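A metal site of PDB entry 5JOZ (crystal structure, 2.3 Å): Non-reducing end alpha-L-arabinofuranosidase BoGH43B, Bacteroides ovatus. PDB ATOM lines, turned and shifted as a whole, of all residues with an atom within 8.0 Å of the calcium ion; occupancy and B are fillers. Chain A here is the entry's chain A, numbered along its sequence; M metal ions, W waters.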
ATOM      1  N   ARG A 311      33.128  -7.896 -16.025  1.00  0.00           N
ATOM      2  CA  ARG A 311      32.184  -6.792 -16.040  1.00  0.00           C
ATOM      3  C   ARG A 311      30.896  -7.125 -15.299  1.00  0.00           C
ATOM      4  O   ARG A 311      30.217  -8.111 -15.624  1.00  0.00           O
ATOM      5  CB  ARG A 311      31.813  -6.457 -17.483  1.00  0.00           C
ATOM      6  CG  ARG A 311      30.855  -5.280 -17.573  1.00  0.00           C
ATOM      7  CD  ARG A 311      30.858  -4.647 -18.952  1.00  0.00           C
ATOM      8  NE  ARG A 311      32.142  -4.050 -19.278  1.00  0.00           N
ATOM      9  CZ  ARG A 311      32.393  -3.331 -20.377  1.00  0.00           C
ATOM     10  NH1 ARG A 311      31.440  -3.080 -21.269  1.00  0.00           N
ATOM     11  NH2 ARG A 311      33.609  -2.835 -20.551  1.00  0.00           N
ATOM     12  N   ASP A 312      30.553  -6.285 -14.325  1.00  0.00           N
ATOM     13  CA  ASP A 312      29.194  -6.215 -13.780  1.00  0.00           C
ATOM     14  C   ASP A 312      28.451  -5.117 -14.552  1.00  0.00           C
ATOM     15  O   ASP A 312      28.766  -3.919 -14.434  1.00  0.00           O
ATOM     16  CB  ASP A 312      29.225  -5.908 -12.274  1.00  0.00           C
ATOM     17  CG  ASP A 312      27.857  -6.075 -11.586  1.00  0.00           C
ATOM     18  OD1 ASP A 312      26.812  -5.981 -12.254  1.00  0.00           O
ATOM     19  OD2 ASP A 312      27.843  -6.256 -10.342  1.00  0.00           O
ATOM     20  N   ASP A 313      27.488  -5.541 -15.357  1.00  0.00           N
ATOM     21  CA  ASP A 313      26.696  -4.628 -16.198  1.00  0.00           C
ATOM     22  C   ASP A 313      25.577  -3.907 -15.425  1.00  0.00           C
ATOM     23  O   ASP A 313      24.902  -3.044 -15.986  1.00  0.00           O
ATOM     24  CB  ASP A 313      26.056  -5.387 -17.383  1.00  0.00           C
ATOM     25  CG  ASP A 313      27.044  -5.728 -18.481  1.00  0.00           C
ATOM     26  OD1 ASP A 313      27.682  -4.802 -19.034  1.00  0.00           O
ATOM     27  OD2 ASP A 313      27.157  -6.923 -18.829  1.00  0.00           O
ATOM     28  N   PHE A 314      25.344  -4.270 -14.161  1.00  0.00           N
ATOM     29  CA  PHE A 314      24.260  -3.651 -13.367  1.00  0.00           C
ATOM     30  C   PHE A 314      22.938  -3.710 -14.129  1.00  0.00           C
ATOM     31  O   PHE A 314      22.214  -2.704 -14.261  1.00  0.00           O
ATOM     32  CB  PHE A 314      24.615  -2.185 -13.012  1.00  0.00           C
ATOM     33  CG  PHE A 314      25.899  -2.026 -12.241  1.00  0.00           C
ATOM     34  CD1 PHE A 314      26.076  -2.663 -11.006  1.00  0.00           C
ATOM     35  CD2 PHE A 314      26.918  -1.217 -12.725  1.00  0.00           C
ATOM     36  CE1 PHE A 314      27.248  -2.512 -10.285  1.00  0.00           C
ATOM     37  CE2 PHE A 314      28.098  -1.050 -11.995  1.00  0.00           C
ATOM     38  CZ  PHE A 314      28.263  -1.697 -10.774  1.00  0.00           C
ATOM     39  N   ASP A 315      22.625  -4.891 -14.652  1.00  0.00           N
ATOM     40  CA  ASP A 315      21.482  -5.068 -15.551  1.00  0.00           C
ATOM     41  C   ASP A 315      20.523  -6.148 -15.033  1.00  0.00           C
ATOM     42  O   ASP A 315      19.865  -6.832 -15.826  1.00  0.00           O
ATOM     43  CB  ASP A 315      21.981  -5.382 -16.978  1.00  0.00           C
ATOM     44  CG  ASP A 315      22.841  -6.650 -17.065  1.00  0.00           C
ATOM     45  OD1 ASP A 315      23.159  -7.250 -16.012  1.00  0.00           O
ATOM     46  OD2 ASP A 315      23.204  -7.041 -18.196  1.00  0.00           O
ATOM     47  N   GLN A 316      20.460  -6.290 -13.706  1.00  0.00           N
ATOM     48  CA  GLN A 316      19.441  -7.089 -13.020  1.00  0.00           C
ATOM     49  C   GLN A 316      19.065  -6.384 -11.709  1.00  0.00           C
ATOM     50  O   GLN A 316      19.848  -5.564 -11.196  1.00  0.00           O
ATOM     51  CB  GLN A 316      19.967  -8.505 -12.738  1.00  0.00           C
ATOM     52  CG  GLN A 316      21.269  -8.529 -11.945  1.00  0.00           C
ATOM     53  CD  GLN A 316      21.786  -9.931 -11.660  1.00  0.00           C
ATOM     54  OE1 GLN A 316      22.037 -10.288 -10.498  1.00  0.00           O
ATOM     55  NE2 GLN A 316      21.949 -10.730 -12.713  1.00  0.00           N
ATOM     56  N   LYS A 339      17.131   3.584 -12.931  1.00  0.00           N
ATOM     57  CA  LYS A 339      17.657   3.632 -14.298  1.00  0.00           C
ATOM     58  C   LYS A 339      18.106   2.235 -14.696  1.00  0.00           C
ATOM     59  O   LYS A 339      19.278   1.906 -14.531  1.00  0.00           O
ATOM     60  CB  LYS A 339      18.801   4.643 -14.406  1.00  0.00           C
ATOM     61  CG  LYS A 339      19.419   4.794 -15.790  1.00  0.00           C
ATOM     62  CD  LYS A 339      18.460   5.398 -16.802  1.00  0.00           C
ATOM     63  CE  LYS A 339      19.042   5.444 -18.211  1.00  0.00           C
ATOM     64  NZ  LYS A 339      20.253   6.303 -18.302  1.00  0.00           N
ATOM     65  N   PRO A 340      17.174   1.388 -15.190  1.00  0.00           N
ATOM     66  CA  PRO A 340      17.527  -0.007 -15.534  1.00  0.00           C
ATOM     67  C   PRO A 340      18.781  -0.088 -16.391  1.00  0.00           C
ATOM     68  O   PRO A 340      18.935   0.677 -17.337  1.00  0.00           O
ATOM     69  CB  PRO A 340      16.302  -0.508 -16.316  1.00  0.00           C
ATOM     70  CG  PRO A 340      15.179   0.408 -15.954  1.00  0.00           C
ATOM     71  CD  PRO A 340      15.792   1.728 -15.575  1.00  0.00           C
ATOM     72  N   GLY A 341      19.686  -0.989 -16.021  1.00  0.00           N
ATOM     73  CA  GLY A 341      20.956  -1.147 -16.732  1.00  0.00           C
ATOM     74  C   GLY A 341      22.080  -0.316 -16.145  1.00  0.00           C
ATOM     75  O   GLY A 341      23.224  -0.438 -16.573  1.00  0.00           O
ATOM     76  N   SER A 342      21.763   0.503 -15.134  1.00  0.00           N
ATOM     77  CA  SER A 342      22.774   1.278 -14.443  1.00  0.00           C
ATOM     78  C   SER A 342      22.625   1.129 -12.944  1.00  0.00           C
ATOM     79  O   SER A 342      21.502   0.968 -12.449  1.00  0.00           O
ATOM     80  CB  SER A 342      22.664   2.754 -14.823  1.00  0.00           C
ATOM     81  OG  SER A 342      23.150   2.968 -16.121  1.00  0.00           O
ATOM     82  N   LEU A 343      23.741   1.200 -12.209  1.00  0.00           N
ATOM     83  CA  LEU A 343      23.683   1.463 -10.771  1.00  0.00           C
ATOM     84  C   LEU A 343      23.660   2.963 -10.560  1.00  0.00           C
ATOM     85  O   LEU A 343      24.637   3.660 -10.873  1.00  0.00           O
ATOM     86  CB  LEU A 343      24.876   0.851 -10.030  1.00  0.00           C
ATOM     87  CG  LEU A 343      24.916   1.158  -8.530  1.00  0.00           C
ATOM     88  CD1 LEU A 343      23.726   0.630  -7.743  1.00  0.00           C
ATOM     89  CD2 LEU A 343      26.203   0.617  -7.972  1.00  0.00           C
ATOM     90  N   LYS A 375      32.316   2.967 -16.244  1.00  0.00           N
ATOM     91  CA  LYS A 375      31.719   3.999 -17.084  1.00  0.00           C
ATOM     92  C   LYS A 375      30.637   4.676 -16.241  1.00  0.00           C
ATOM     93  O   LYS A 375      29.720   4.011 -15.747  1.00  0.00           O
ATOM     94  CB  LYS A 375      31.111   3.361 -18.335  1.00  0.00           C
ATOM     95  CG  LYS A 375      30.622   4.310 -19.427  1.00  0.00           C
ATOM     96  CD  LYS A 375      29.492   3.648 -20.221  1.00  0.00           C
ATOM     97  CE  LYS A 375      29.407   4.131 -21.656  1.00  0.00           C
ATOM     98  NZ  LYS A 375      28.229   3.513 -22.334  1.00  0.00           N
ATOM     99  N   PHE A 498      26.282   4.576 -12.980  1.00  0.00           N
ATOM    100  CA  PHE A 498      27.367   3.688 -13.381  1.00  0.00           C
ATOM    101  C   PHE A 498      26.784   2.605 -14.277  1.00  0.00           C
ATOM    102  O   PHE A 498      26.054   1.741 -13.802  1.00  0.00           O
ATOM    103  CB  PHE A 498      28.034   3.064 -12.156  1.00  0.00           C
ATOM    104  CG  PHE A 498      28.742   4.076 -11.303  1.00  0.00           C
ATOM    105  CD1 PHE A 498      28.040   4.855 -10.407  1.00  0.00           C
ATOM    106  CD2 PHE A 498      30.102   4.279 -11.430  1.00  0.00           C
ATOM    107  CE1 PHE A 498      28.693   5.795  -9.625  1.00  0.00           C
ATOM    108  CE2 PHE A 498      30.767   5.213 -10.646  1.00  0.00           C
ATOM    109  CZ  PHE A 498      30.067   5.964  -9.746  1.00  0.00           C
ATOM    110  N   ASP A 499      27.115   2.670 -15.555  1.00  0.00           N
ATOM    111  CA  ASP A 499      26.609   1.714 -16.543  1.00  0.00           C
ATOM    112  C   ASP A 499      27.246   0.338 -16.316  1.00  0.00           C
ATOM    113  O   ASP A 499      26.567  -0.682 -16.402  1.00  0.00           O
ATOM    114  CB  ASP A 499      26.929   2.216 -17.953  1.00  0.00           C
ATOM    115  CG  ASP A 499      26.154   1.501 -19.038  1.00  0.00           C
ATOM    116  OD1 ASP A 499      25.310   0.625 -18.734  1.00  0.00           O
ATOM    117  OD2 ASP A 499      26.384   1.819 -20.219  1.00  0.00           O
ATOM    118  N   TRP A 500      28.539   0.313 -16.043  1.00  0.00           N
ATOM    119  CA  TRP A 500      29.212  -0.932 -15.726  1.00  0.00           C
ATOM    120  C   TRP A 500      30.437  -0.707 -14.872  1.00  0.00           C
ATOM    121  O   TRP A 500      30.851   0.431 -14.665  1.00  0.00           O
ATOM    122  CB  TRP A 500      29.549  -1.726 -16.999  1.00  0.00           C
ATOM    123  CG  TRP A 500      30.218  -0.949 -18.109  1.00  0.00           C
ATOM    124  CD1 TRP A 500      29.615  -0.487 -19.251  1.00  0.00           C
ATOM    125  CD2 TRP A 500      31.590  -0.574 -18.197  1.00  0.00           C
ATOM    126  NE1 TRP A 500      30.528   0.154 -20.034  1.00  0.00           N
ATOM    127  CE2 TRP A 500      31.758   0.106 -19.423  1.00  0.00           C
ATOM    128  CE3 TRP A 500      32.701  -0.770 -17.380  1.00  0.00           C
ATOM    129  CZ2 TRP A 500      33.000   0.606 -19.850  1.00  0.00           C
ATOM    130  CZ3 TRP A 500      33.947  -0.259 -17.786  1.00  0.00           C
ATOM    131  CH2 TRP A 500      34.069   0.441 -19.008  1.00  0.00           C
ATOM    132  N   PHE A 501      30.988  -1.807 -14.359  1.00  0.00           N
ATOM    133  CA  PHE A 501      32.177  -1.813 -13.503  1.00  0.00           C
ATOM    134  C   PHE A 501      32.962  -3.097 -13.807  1.00  0.00           C
ATOM    135  O   PHE A 501      32.447  -4.196 -13.580  1.00  0.00           O
ATOM    136  CB  PHE A 501      31.760  -1.787 -12.027  1.00  0.00           C
ATOM    137  CG  PHE A 501      32.901  -1.544 -11.068  1.00  0.00           C
ATOM    138  CD1 PHE A 501      33.823  -2.545 -10.753  1.00  0.00           C
ATOM    139  CD2 PHE A 501      33.034  -0.299 -10.441  1.00  0.00           C
ATOM    140  CE1 PHE A 501      34.860  -2.311  -9.867  1.00  0.00           C
ATOM    141  CE2 PHE A 501      34.075  -0.057  -9.550  1.00  0.00           C
ATOM    142  CZ  PHE A 501      34.980  -1.063  -9.257  1.00  0.00           C
HETATM  143 CA    CA M   1      24.876  -1.558 -17.807  1.00  0.00          CA
HETATM  144  O   HOH W   1      23.212  -2.735 -19.137  1.00  0.00           O
HETATM  145  O   HOH W   2      26.615  -2.459 -19.194  1.00  0.00           O
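The side-chain carboxylate of Asp 499 is in salt-bridge range of the side-chain amino group of Lys 375 (3.3 Å).
O of Gly 341 binds the calcium ion (2.3 Å). The backbone carbonyl oxygen (O) of Asp 313 is bound to the calcium ion, at 2.4 Å. The calcium ion is bound by O of Asp 499, at 2.4 Å. Water W2 binds the calcium ion, 2.4 Å away. The calcium ion is bound by the side-chain carboxylate (OD1) of Asp 499, at 2.4 Å. The calcium ion is bound by water W1.
Of the 16 residues printed, 3 come within 4 Å of the calcium ion. Along chain A the residues within 4 Å of the calcium ion span positions 313 to 499. The nearest printed residue that does not touch the calcium ion is Trp 500 (4.5 Å).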
